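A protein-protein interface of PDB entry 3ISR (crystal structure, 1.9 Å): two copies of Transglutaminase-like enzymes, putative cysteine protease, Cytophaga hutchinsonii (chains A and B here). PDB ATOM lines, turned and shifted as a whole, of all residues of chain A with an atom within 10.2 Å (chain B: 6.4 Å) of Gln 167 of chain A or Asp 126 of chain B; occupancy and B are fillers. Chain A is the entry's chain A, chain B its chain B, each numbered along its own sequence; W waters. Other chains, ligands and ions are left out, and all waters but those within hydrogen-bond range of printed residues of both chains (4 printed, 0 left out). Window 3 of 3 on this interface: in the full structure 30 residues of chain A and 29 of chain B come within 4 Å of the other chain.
Of the 12 printed residues of chain B, 5 touch a printed residue of chain A. Hydrophobic or aromatic side chains of chain B that line the printed part of chain A: Pro 119. Hydrophobic or aromatic side chains of chain A within 4 Å of the printed part of chain B: Tyr 122 and Ala 250. Among the printed residues, 10 pairs touch across the chains.
Among the printed residues, merely in contact across the chains: Arg 121 of chain A with Ser 120 of chain B (3.5 Å), Ala 250 of chain A with Pro 119 of chain B (3.6 Å), Gln 167 of chain A with Lys 127 of chain B (3.6 Å), Arg 121 of chain A with Lys 127 of chain B (3.6 Å), Arg 121 of chain A with Pro 119 of chain B (3.7 Å), Arg 121 of chain A with Gln 124 of chain B (3.8 Å) and Ser 166 of chain A with Asp 126 of chain B (3.9 Å).
Gln 167 of chain A touches just these residues of chain B: Asp 126 (3.3 Å) and Lys 127 (3.6 Å). Asp 126 of chain B touches four residues of chain A. Ser 125 of chain B touches none of the printed residues of chain A. Lys 127 of chain B touches just these residues of chain A: Arg 121 and Gln 167. Of the printed residues of chain B, Ser 166 of chain A touches Asp 126 (3.9 Å). Of the printed residues of chain A, Pro 119 of chain B touches Arg 121 and Ala 250. Of the printed residues of chain A, Ser 120 of chain B touches Arg 121 (3.5 Å). Thr 164 of chain A touches none of the printed residues of chain B.
The guanidinium group (NE) of Arg 121 of chain A lies within salt-bridge range of the side-chain carboxylate (OD1) of Asp 126 of chain B (2.8 Å). The side-chain hydroxyl (OH) of Tyr 122 of chain A sits at hydrogen-bond distance from the side-chain carboxylate (OD2) of Asp 126 of chain B. The side-chain amide nitrogen (NE2) of Gln 167 of chain A lies within hydrogen-bond range of the backbone carbonyl oxygen (O) of Asp 126 of chain B (3.3 Å).
Water W1 lies within hydrogen-bond range of OD2 of Asp 126 of chain B, O of Ser 166 of chain A and OH of Tyr 122 of chain A. Water W4 lies within hydrogen-bond range of OD2 of Asp 172 of chain A, NZ of Lys 127 of chain B and O of Gln 167 of chain A. Water W2 lies within hydrogen-bond range of the backbone carbonyl oxygen (O) of Gln 167 of chain A, the guanidinium group (NH1) of Arg 121 of chain A, the side-chain hydroxyl (OG) of Ser 169 of chain A, the side-chain amino group (NZ) of Lys 127 of chain B and the side-chain carboxylate (OD2) of Asp 172 of chain A. Water W3 bridges the side-chain amide nitrogen of Gln 124 of chain A and the side-chain amide nitrogen of Gln 124 of chain B.
Positions printed for both chains: 120, 123 and 124.
NH2 of Arg 121 of chain A sits at hydrogen-bond distance from O of Gln 167 of chain A (3.1 Å). OD2 of Asp 248 of chain A lies within hydrogen-bond range of N of Arg 121 of chain A, 3.0 Å away. The side-chain carboxylate of Asp 248 of chain A lies within hydrogen-bond range of the backbone NH of Tyr 122 of chain A, at 2.8 Å. O of Ser 166 of chain A lies within hydrogen-bond range of NH2 of Arg 182 of chain A (2.9 Å). The side-chain carboxylate (OD1) of Asp 248 of chain A sits at hydrogen-bond distance from the backbone NH (N) of Ala 250 of chain A. OG of Ser 120 of chain B sits close to SG of Cys 123 of chain B.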
ATOM      1  N   SER A 120     -20.530  17.603  32.693  1.00  0.00           N
ATOM      2  CA  SER A 120     -21.354  17.594  31.488  1.00  0.00           C
ATOM      3  C   SER A 120     -21.357  19.000  30.876  1.00  0.00           C
ATOM      4  O   SER A 120     -20.709  19.909  31.411  1.00  0.00           O
ATOM      5  CB  SER A 120     -22.764  17.113  31.830  1.00  0.00           C
ATOM      6  OG  SER A 120     -23.365  17.969  32.789  1.00  0.00           O
ATOM      7  N   ARG A 121     -22.077  19.190  29.769  1.00  0.00           N
ATOM      8  CA  ARG A 121     -22.030  20.470  29.045  1.00  0.00           C
ATOM      9  C   ARG A 121     -22.228  21.690  29.969  1.00  0.00           C
ATOM     10  O   ARG A 121     -21.456  22.655  29.925  1.00  0.00           O
ATOM     11  CB  ARG A 121     -23.093  20.482  27.937  1.00  0.00           C
ATOM     12  CG  ARG A 121     -23.362  21.876  27.346  1.00  0.00           C
ATOM     13  CD  ARG A 121     -22.144  22.531  26.606  1.00  0.00           C
ATOM     14  NE  ARG A 121     -22.535  23.874  26.140  1.00  0.00           N
ATOM     15  CZ  ARG A 121     -22.416  25.005  26.847  1.00  0.00           C
ATOM     16  NH1 ARG A 121     -21.883  24.996  28.074  1.00  0.00           N
ATOM     17  NH2 ARG A 121     -22.848  26.160  26.334  1.00  0.00           N
ATOM     18  N   TYR A 122     -23.298  21.648  30.762  1.00  0.00           N
ATOM     19  CA  TYR A 122     -23.675  22.770  31.628  1.00  0.00           C
ATOM     20  C   TYR A 122     -23.186  22.664  33.060  1.00  0.00           C
ATOM     21  O   TYR A 122     -23.545  23.517  33.886  1.00  0.00           O
ATOM     22  CB  TYR A 122     -25.201  23.016  31.585  1.00  0.00           C
ATOM     23  CG  TYR A 122     -25.664  23.249  30.178  1.00  0.00           C
ATOM     24  CD1 TYR A 122     -25.324  24.423  29.497  1.00  0.00           C
ATOM     25  CD2 TYR A 122     -26.379  22.269  29.499  1.00  0.00           C
ATOM     26  CE1 TYR A 122     -25.725  24.637  28.174  1.00  0.00           C
ATOM     27  CE2 TYR A 122     -26.792  22.462  28.180  1.00  0.00           C
ATOM     28  CZ  TYR A 122     -26.463  23.646  27.538  1.00  0.00           C
ATOM     29  OH  TYR A 122     -26.852  23.806  26.250  1.00  0.00           O
ATOM     30  N   CYS A 123     -22.391  21.628  33.362  1.00  0.00           N
ATOM     31  CA  CYS A 123     -21.962  21.333  34.741  1.00  0.00           C
ATOM     32  C   CYS A 123     -20.482  20.974  34.732  1.00  0.00           C
ATOM     33  O   CYS A 123     -20.118  19.805  34.795  1.00  0.00           O
ATOM     34  CB  CYS A 123     -22.789  20.160  35.358  1.00  0.00           C
ATOM     35  SG  CYS A 123     -24.574  20.430  35.253  1.00  0.00           S
ATOM     36  N   GLN A 124     -19.642  21.998  34.656  1.00  0.00           N
ATOM     37  CA  GLN A 124     -18.186  21.815  34.531  1.00  0.00           C
ATOM     38  C   GLN A 124     -17.598  21.595  35.919  1.00  0.00           C
ATOM     39  O   GLN A 124     -16.816  22.396  36.427  1.00  0.00           O
ATOM     40  CB  GLN A 124     -17.551  23.038  33.834  1.00  0.00           C
ATOM     41  CG  GLN A 124     -18.243  23.425  32.498  1.00  0.00           C
ATOM     42  CD  GLN A 124     -19.277  24.535  32.651  1.00  0.00           C
ATOM     43  OE1 GLN A 124     -20.049  24.567  33.616  1.00  0.00           O
ATOM     44  NE2 GLN A 124     -19.300  25.448  31.685  1.00  0.00           N
ATOM     45  N   SER A 163     -32.231  36.702  32.757  1.00  0.00           N
ATOM     46  CA  SER A 163     -30.831  37.047  33.030  1.00  0.00           C
ATOM     47  C   SER A 163     -29.861  36.081  32.347  1.00  0.00           C
ATOM     48  O   SER A 163     -28.657  36.338  32.294  1.00  0.00           O
ATOM     49  CB  SER A 163     -30.550  37.044  34.537  1.00  0.00           C
ATOM     50  OG  SER A 163     -30.834  35.781  35.096  1.00  0.00           O
ATOM     51  N   THR A 164     -30.381  34.953  31.870  1.00  0.00           N
ATOM     52  CA  THR A 164     -29.532  33.913  31.298  1.00  0.00           C
ATOM     53  C   THR A 164     -30.113  33.395  29.976  1.00  0.00           C
ATOM     54  O   THR A 164     -31.209  33.783  29.565  1.00  0.00           O
ATOM     55  CB  THR A 164     -29.331  32.717  32.279  1.00  0.00           C
ATOM     56  OG1 THR A 164     -30.592  32.133  32.588  1.00  0.00           O
ATOM     57  CG2 THR A 164     -28.647  33.142  33.593  1.00  0.00           C
ATOM     58  N   ASN A 165     -29.374  32.513  29.306  1.00  0.00           N
ATOM     59  CA  ASN A 165     -29.886  31.885  28.102  1.00  0.00           C
ATOM     60  C   ASN A 165     -29.496  30.410  28.047  1.00  0.00           C
ATOM     61  O   ASN A 165     -28.945  29.880  29.002  1.00  0.00           O
ATOM     62  CB  ASN A 165     -29.387  32.628  26.865  1.00  0.00           C
ATOM     63  CG  ASN A 165     -27.871  32.683  26.788  1.00  0.00           C
ATOM     64  OD1 ASN A 165     -27.178  31.719  27.118  1.00  0.00           O
ATOM     65  ND2 ASN A 165     -27.346  33.820  26.329  1.00  0.00           N
ATOM     66  N   SER A 166     -29.761  29.756  26.920  1.00  0.00           N
ATOM     67  CA  SER A 166     -29.546  28.319  26.854  1.00  0.00           C
ATOM     68  C   SER A 166     -28.055  27.933  26.807  1.00  0.00           C
ATOM     69  O   SER A 166     -27.729  26.760  26.963  1.00  0.00           O
ATOM     70  CB  SER A 166     -30.298  27.692  25.675  1.00  0.00           C
ATOM     71  OG  SER A 166     -29.758  28.141  24.449  1.00  0.00           O
ATOM     72  N   GLN A 167     -27.165  28.899  26.610  1.00  0.00           N
ATOM     73  CA  GLN A 167     -25.731  28.609  26.612  1.00  0.00           C
ATOM     74  C   GLN A 167     -25.134  28.699  28.008  1.00  0.00           C
ATOM     75  O   GLN A 167     -24.018  28.243  28.242  1.00  0.00           O
ATOM     76  CB  GLN A 167     -24.980  29.552  25.666  1.00  0.00           C
ATOM     77  CG  GLN A 167     -25.415  29.411  24.206  1.00  0.00           C
ATOM     78  CD  GLN A 167     -24.704  30.394  23.300  1.00  0.00           C
ATOM     79  OE1 GLN A 167     -23.731  31.024  23.700  1.00  0.00           O
ATOM     80  NE2 GLN A 167     -25.186  30.527  22.077  1.00  0.00           N
ATOM     81  N   THR A 168     -25.870  29.313  28.930  1.00  0.00           N
ATOM     82  CA  THR A 168     -25.379  29.545  30.290  1.00  0.00           C
ATOM     83  C   THR A 168     -25.148  28.220  31.023  1.00  0.00           C
ATOM     84  O   THR A 168     -25.968  27.301  30.935  1.00  0.00           O
ATOM     85  CB  THR A 168     -26.402  30.384  31.116  1.00  0.00           C
ATOM     86  OG1 THR A 168     -26.686  31.617  30.425  1.00  0.00           O
ATOM     87  CG2 THR A 168     -25.880  30.663  32.520  1.00  0.00           C
ATOM     88  N   SER A 169     -24.059  28.173  31.781  1.00  0.00           N
ATOM     89  CA  SER A 169     -23.639  26.986  32.521  1.00  0.00           C
ATOM     90  C   SER A 169     -23.407  27.287  34.001  1.00  0.00           C
ATOM     91  O   SER A 169     -23.401  28.459  34.427  1.00  0.00           O
ATOM     92  CB  SER A 169     -22.344  26.432  31.908  1.00  0.00           C
ATOM     93  OG  SER A 169     -21.265  27.330  32.134  1.00  0.00           O
ATOM     94  N   ALA A 170     -23.212  26.234  34.786  1.00  0.00           N
ATOM     95  CA  ALA A 170     -22.891  26.378  36.220  1.00  0.00           C
ATOM     96  C   ALA A 170     -21.654  27.261  36.418  1.00  0.00           C
ATOM     97  O   ALA A 170     -21.605  28.074  37.338  1.00  0.00           O
ATOM     98  CB  ALA A 170     -22.674  24.973  36.866  1.00  0.00           C
ATOM     99  N   PHE A 171     -20.670  27.101  35.542  1.00  0.00           N
ATOM    100  CA  PHE A 171     -19.410  27.866  35.632  1.00  0.00           C
ATOM    101  C   PHE A 171     -19.672  29.366  35.485  1.00  0.00           C
ATOM    102  O   PHE A 171     -19.005  30.186  36.131  1.00  0.00           O
ATOM    103  CB  PHE A 171     -18.396  27.387  34.581  1.00  0.00           C
ATOM    104  CG  PHE A 171     -17.020  27.948  34.769  1.00  0.00           C
ATOM    105  CD1 PHE A 171     -16.179  27.455  35.776  1.00  0.00           C
ATOM    106  CD2 PHE A 171     -16.554  28.979  33.944  1.00  0.00           C
ATOM    107  CE1 PHE A 171     -14.883  27.975  35.950  1.00  0.00           C
ATOM    108  CE2 PHE A 171     -15.261  29.507  34.124  1.00  0.00           C
ATOM    109  CZ  PHE A 171     -14.426  28.991  35.123  1.00  0.00           C
ATOM    110  N   ASP A 172     -20.644  29.717  34.645  1.00  0.00           N
ATOM    111  CA  ASP A 172     -21.081  31.109  34.504  1.00  0.00           C
ATOM    112  C   ASP A 172     -21.821  31.641  35.730  1.00  0.00           C
ATOM    113  O   ASP A 172     -21.548  32.746  36.205  1.00  0.00           O
ATOM    114  CB  ASP A 172     -21.991  31.249  33.290  1.00  0.00           C
ATOM    115  CG  ASP A 172     -21.333  30.776  32.009  1.00  0.00           C
ATOM    116  OD1 ASP A 172     -20.128  31.060  31.812  1.00  0.00           O
ATOM    117  OD2 ASP A 172     -22.027  30.148  31.185  1.00  0.00           O
ATOM    118  N   THR A 173     -22.742  30.839  36.243  1.00  0.00           N
ATOM    119  CA  THR A 173     -23.630  31.264  37.331  1.00  0.00           C
ATOM    120  C   THR A 173     -22.865  31.550  38.622  1.00  0.00           C
ATOM    121  O   THR A 173     -23.235  32.445  39.382  1.00  0.00           O
ATOM    122  CB  THR A 173     -24.749  30.222  37.535  1.00  0.00           C
ATOM    123  OG1 THR A 173     -25.440  30.071  36.292  1.00  0.00           O
ATOM    124  CG2 THR A 173     -25.782  30.681  38.612  1.00  0.00           C
ATOM    125  N   GLU A 176     -21.693  35.076  37.878  1.00  0.00           N
ATOM    126  CA  GLU A 176     -22.798  35.968  37.519  1.00  0.00           C
ATOM    127  C   GLU A 176     -23.764  36.205  38.677  1.00  0.00           C
ATOM    128  O   GLU A 176     -24.279  37.320  38.842  1.00  0.00           O
ATOM    129  CB  GLU A 176     -23.556  35.437  36.290  1.00  0.00           C
ATOM    130  CG  GLU A 176     -22.737  35.594  34.974  1.00  0.00           C
ATOM    131  CD  GLU A 176     -23.362  34.882  33.741  1.00  0.00           C
ATOM    132  OE1 GLU A 176     -24.458  34.248  33.858  1.00  0.00           O
ATOM    133  OE2 GLU A 176     -22.756  34.992  32.642  1.00  0.00           O
ATOM    134  N   VAL A 180     -32.172  31.529  36.404  1.00  0.00           N
ATOM    135  CA  VAL A 180     -33.490  30.905  36.608  1.00  0.00           C
ATOM    136  C   VAL A 180     -33.337  29.419  36.976  1.00  0.00           C
ATOM    137  O   VAL A 180     -32.209  28.967  37.214  1.00  0.00           O
ATOM    138  CB  VAL A 180     -34.386  31.113  35.389  1.00  0.00           C
ATOM    139  CG1 VAL A 180     -34.803  32.604  35.288  1.00  0.00           C
ATOM    140  CG2 VAL A 180     -33.699  30.629  34.129  1.00  0.00           C
ATOM    141  N   ARG A 182     -33.272  26.465  35.674  1.00  0.00           N
ATOM    142  CA  ARG A 182     -32.306  25.627  34.942  1.00  0.00           C
ATOM    143  C   ARG A 182     -30.864  25.899  35.425  1.00  0.00           C
ATOM    144  O   ARG A 182     -30.050  24.970  35.587  1.00  0.00           O
ATOM    145  CB  ARG A 182     -32.460  25.941  33.465  1.00  0.00           C
ATOM    146  CG  ARG A 182     -31.486  25.273  32.505  1.00  0.00           C
ATOM    147  CD  ARG A 182     -31.622  26.047  31.201  1.00  0.00           C
ATOM    148  NE  ARG A 182     -31.071  25.408  30.006  1.00  0.00           N
ATOM    149  CZ  ARG A 182     -29.808  25.494  29.582  1.00  0.00           C
ATOM    150  NH1 ARG A 182     -28.869  26.131  30.307  1.00  0.00           N
ATOM    151  NH2 ARG A 182     -29.488  24.906  28.426  1.00  0.00           N
ATOM    152  N   ASP A 183     -30.549  27.178  35.655  1.00  0.00           N
ATOM    153  CA  ASP A 183     -29.224  27.541  36.147  1.00  0.00           C
ATOM    154  C   ASP A 183     -29.010  27.123  37.580  1.00  0.00           C
ATOM    155  O   ASP A 183     -27.911  26.713  37.931  1.00  0.00           O
ATOM    156  CB  ASP A 183     -28.981  29.051  36.019  1.00  0.00           C
ATOM    157  CG  ASP A 183     -29.343  29.560  34.657  1.00  0.00           C
ATOM    158  OD1 ASP A 183     -28.740  29.068  33.676  1.00  0.00           O
ATOM    159  OD2 ASP A 183     -30.254  30.429  34.555  1.00  0.00           O
ATOM    160  N   HIS A 186     -28.335  23.315  37.400  1.00  0.00           N
ATOM    161  CA  HIS A 186     -26.994  22.998  36.897  1.00  0.00           C
ATOM    162  C   HIS A 186     -25.925  23.331  37.932  1.00  0.00           C
ATOM    163  O   HIS A 186     -24.952  22.616  38.070  1.00  0.00           O
ATOM    164  CB  HIS A 186     -26.668  23.801  35.626  1.00  0.00           C
ATOM    165  CG  HIS A 186     -27.431  23.375  34.396  1.00  0.00           C
ATOM    166  ND1 HIS A 186     -27.796  22.069  34.135  1.00  0.00           N
ATOM    167  CD2 HIS A 186     -27.869  24.099  33.344  1.00  0.00           C
ATOM    168  CE1 HIS A 186     -28.414  22.006  32.964  1.00  0.00           C
ATOM    169  NE2 HIS A 186     -28.481  23.229  32.470  1.00  0.00           N
ATOM    170  N   ASP A 248     -27.763  16.743  32.369  1.00  0.00           N
ATOM    171  CA  ASP A 248     -28.084  18.174  32.460  1.00  0.00           C
ATOM    172  C   ASP A 248     -29.126  18.472  31.393  1.00  0.00           C
ATOM    173  O   ASP A 248     -29.623  17.537  30.772  1.00  0.00           O
ATOM    174  CB  ASP A 248     -26.834  19.095  32.355  1.00  0.00           C
ATOM    175  CG  ASP A 248     -26.063  18.958  31.040  1.00  0.00           C
ATOM    176  OD1 ASP A 248     -26.646  18.568  30.025  1.00  0.00           O
ATOM    177  OD2 ASP A 248     -24.846  19.319  31.019  1.00  0.00           O
ATOM    178  N   ALA A 249     -29.410  19.756  31.162  1.00  0.00           N
ATOM    179  CA  ALA A 249     -30.457  20.198  30.216  1.00  0.00           C
ATOM    180  C   ALA A 249     -30.239  19.735  28.787  1.00  0.00           C
ATOM    181  O   ALA A 249     -31.182  19.697  28.039  1.00  0.00           O
ATOM    182  CB  ALA A 249     -30.608  21.743  30.226  1.00  0.00           C
ATOM    183  N   ALA A 250     -29.008  19.394  28.406  1.00  0.00           N
ATOM    184  CA  ALA A 250     -28.750  18.892  27.046  1.00  0.00           C
ATOM    185  C   ALA A 250     -29.510  17.581  26.804  1.00  0.00           C
ATOM    186  O   ALA A 250     -29.836  17.243  25.662  1.00  0.00           O
ATOM    187  CB  ALA A 250     -27.221  18.685  26.810  1.00  0.00           C
ATOM    188  N   SER A 256     -36.338  20.724  21.230  1.00  0.00           N
ATOM    189  CA  SER A 256     -35.165  20.854  20.396  1.00  0.00           C
ATOM    190  C   SER A 256     -35.647  21.090  18.967  1.00  0.00           C
ATOM    191  O   SER A 256     -36.427  20.306  18.433  1.00  0.00           O
ATOM    192  CB  SER A 256     -34.291  19.603  20.487  1.00  0.00           C
ATOM    193  OG  SER A 256     -33.768  19.490  21.804  1.00  0.00           O
ATOM    194  N   PRO B 119     -24.865  19.176  22.634  1.00  0.00           N
ATOM    195  CA  PRO B 119     -23.577  19.593  23.210  1.00  0.00           C
ATOM    196  C   PRO B 119     -23.215  18.702  24.390  1.00  0.00           C
ATOM    197  O   PRO B 119     -24.119  18.170  25.077  1.00  0.00           O
ATOM    198  CB  PRO B 119     -23.842  21.016  23.711  1.00  0.00           C
ATOM    199  CG  PRO B 119     -25.205  21.429  23.174  1.00  0.00           C
ATOM    200  CD  PRO B 119     -25.927  20.201  22.748  1.00  0.00           C
ATOM    201  N   SER B 120     -21.919  18.560  24.650  1.00  0.00           N
ATOM    202  CA  SER B 120     -21.438  17.817  25.798  1.00  0.00           C
ATOM    203  C   SER B 120     -20.354  18.641  26.512  1.00  0.00           C
ATOM    204  O   SER B 120     -20.047  19.743  26.069  1.00  0.00           O
ATOM    205  CB  SER B 120     -20.885  16.472  25.328  1.00  0.00           C
ATOM    206  OG  SER B 120     -19.854  16.662  24.387  1.00  0.00           O
ATOM    207  N   CYS B 123     -17.554  19.655  24.146  1.00  0.00           N
ATOM    208  CA  CYS B 123     -17.983  19.915  22.768  1.00  0.00           C
ATOM    209  C   CYS B 123     -19.198  20.847  22.811  1.00  0.00           C
ATOM    210  O   CYS B 123     -20.356  20.400  22.701  1.00  0.00           O
ATOM    211  CB  CYS B 123     -18.332  18.614  22.031  1.00  0.00           C
ATOM    212  SG  CYS B 123     -17.036  17.366  22.026  1.00  0.00           S
ATOM    213  N   GLN B 124     -18.922  22.148  22.983  1.00  0.00           N
ATOM    214  CA  GLN B 124     -19.979  23.171  23.166  1.00  0.00           C
ATOM    215  C   GLN B 124     -20.509  23.629  21.817  1.00  0.00           C
ATOM    216  O   GLN B 124     -20.299  24.780  21.375  1.00  0.00           O
ATOM    217  CB  GLN B 124     -19.454  24.350  23.991  1.00  0.00           C
ATOM    218  CG  GLN B 124     -18.800  23.956  25.341  1.00  0.00           C
ATOM    219  CD  GLN B 124     -17.282  23.867  25.249  1.00  0.00           C
ATOM    220  OE1 GLN B 124     -16.723  23.408  24.235  1.00  0.00           O
ATOM    221  NE2 GLN B 124     -16.600  24.317  26.305  1.00  0.00           N
ATOM    222  N   SER B 125     -21.198  22.708  21.151  1.00  0.00           N
ATOM    223  CA  SER B 125     -21.644  22.904  19.790  1.00  0.00           C
ATOM    224  C   SER B 125     -22.653  24.025  19.729  1.00  0.00           C
ATOM    225  O   SER B 125     -22.750  24.743  18.732  1.00  0.00           O
ATOM    226  CB  SER B 125     -22.247  21.603  19.226  1.00  0.00           C
ATOM    227  OG  SER B 125     -23.073  20.954  20.189  1.00  0.00           O
ATOM    228  N   ASP B 126     -23.376  24.207  20.826  1.00  0.00           N
ATOM    229  CA  ASP B 126     -24.357  25.282  20.885  1.00  0.00           C
ATOM    230  C   ASP B 126     -23.711  26.680  20.892  1.00  0.00           C
ATOM    231  O   ASP B 126     -24.380  27.648  20.590  1.00  0.00           O
ATOM    232  CB  ASP B 126     -25.291  25.086  22.099  1.00  0.00           C
ATOM    233  CG  ASP B 126     -24.545  25.087  23.430  1.00  0.00           C
ATOM    234  OD1 ASP B 126     -23.500  24.423  23.549  1.00  0.00           O
ATOM    235  OD2 ASP B 126     -25.017  25.762  24.369  1.00  0.00           O
ATOM    236  N   LYS B 127     -22.435  26.797  21.252  1.00  0.00           N
ATOM    237  CA  LYS B 127     -21.750  28.101  21.209  1.00  0.00           C
ATOM    238  C   LYS B 127     -21.051  28.353  19.879  1.00  0.00           C
ATOM    239  O   LYS B 127     -20.440  29.413  19.668  1.00  0.00           O
ATOM    240  CB  LYS B 127     -20.731  28.215  22.338  1.00  0.00           C
ATOM    241  CG  LYS B 127     -21.386  28.255  23.734  1.00  0.00           C
ATOM    242  CD  LYS B 127     -20.340  28.402  24.835  1.00  0.00           C
ATOM    243  CE  LYS B 127     -20.413  29.754  25.525  1.00  0.00           C
ATOM    244  NZ  LYS B 127     -19.628  29.730  26.798  1.00  0.00           N
ATOM    245  N   LEU B 128     -21.119  27.368  19.001  1.00  0.00           N
ATOM    246  CA  LEU B 128     -20.346  27.416  17.751  1.00  0.00           C
ATOM    247  C   LEU B 128     -21.206  27.351  16.485  1.00  0.00           C
ATOM    248  O   LEU B 128     -20.676  27.181  15.392  1.00  0.00           O
ATOM    249  CB  LEU B 128     -19.291  26.286  17.757  1.00  0.00           C
ATOM    250  CG  LEU B 128     -18.209  26.393  18.839  1.00  0.00           C
ATOM    251  CD1 LEU B 128     -17.323  25.145  18.878  1.00  0.00           C
ATOM    252  CD2 LEU B 128     -17.349  27.637  18.639  1.00  0.00           C
ATOM    253  N   GLN B 129     -22.520  27.522  16.618  1.00  0.00           N
ATOM    254  CA  GLN B 129     -23.415  27.413  15.451  1.00  0.00           C
ATOM    255  C   GLN B 129     -23.147  28.470  14.355  1.00  0.00           C
ATOM    256  O   GLN B 129     -23.065  28.137  13.172  1.00  0.00           O
ATOM    257  CB  GLN B 129     -24.895  27.488  15.868  1.00  0.00           C
ATOM    258  CG  GLN B 129     -25.365  26.430  16.858  1.00  0.00           C
ATOM    259  CD  GLN B 129     -26.798  26.693  17.343  1.00  0.00           C
ATOM    260  OE1 GLN B 129     -27.756  26.474  16.606  1.00  0.00           O
ATOM    261  NE2 GLN B 129     -26.939  27.170  18.587  1.00  0.00           N
ATOM    262  N   LYS B 130     -23.022  29.742  14.742  1.00  0.00           N
ATOM    263  CA  LYS B 130     -22.784  30.792  13.738  1.00  0.00           C
ATOM    264  C   LYS B 130     -21.466  30.597  13.059  1.00  0.00           C
ATOM    265  O   LYS B 130     -21.385  30.680  11.844  1.00  0.00           O
ATOM    266  CB  LYS B 130     -22.843  32.185  14.343  1.00  0.00           C
ATOM    267  CG  LYS B 130     -24.198  32.808  14.229  1.00  0.00           C
ATOM    268  CD  LYS B 130     -24.146  34.283  14.565  1.00  0.00           C
ATOM    269  CE  LYS B 130     -25.543  34.820  14.786  1.00  0.00           C
ATOM    270  NZ  LYS B 130     -26.367  34.678  13.544  1.00  0.00           N
ATOM    271  N   ALA B 190     -17.587  18.924  17.903  1.00  0.00           N
ATOM    272  CA  ALA B 190     -18.362  20.136  18.165  1.00  0.00           C
ATOM    273  C   ALA B 190     -18.828  20.781  16.881  1.00  0.00           C
ATOM    274  O   ALA B 190     -19.966  21.204  16.789  1.00  0.00           O
ATOM    275  CB  ALA B 190     -17.556  21.146  19.002  1.00  0.00           C
ATOM    276  N   ALA B 194     -22.645  21.220  15.564  1.00  0.00           N
ATOM    277  CA  ALA B 194     -23.090  22.607  15.341  1.00  0.00           C
ATOM    278  C   ALA B 194     -23.849  22.713  14.022  1.00  0.00           C
ATOM    279  O   ALA B 194     -24.706  23.594  13.848  1.00  0.00           O
ATOM    280  CB  ALA B 194     -21.877  23.539  15.354  1.00  0.00           C
HETATM  281  O   HOH W   1     -27.600  26.197  24.096  1.00  0.00           O
HETATM  282  O   HOH W   2     -21.186  27.775  28.989  1.00  0.00           O
HETATM  283  O   HOH W   3     -17.688  25.215  29.119  1.00  0.00           O
HETATM  284  O   HOH W   4     -21.764  30.783  28.493  1.00  0.00           O
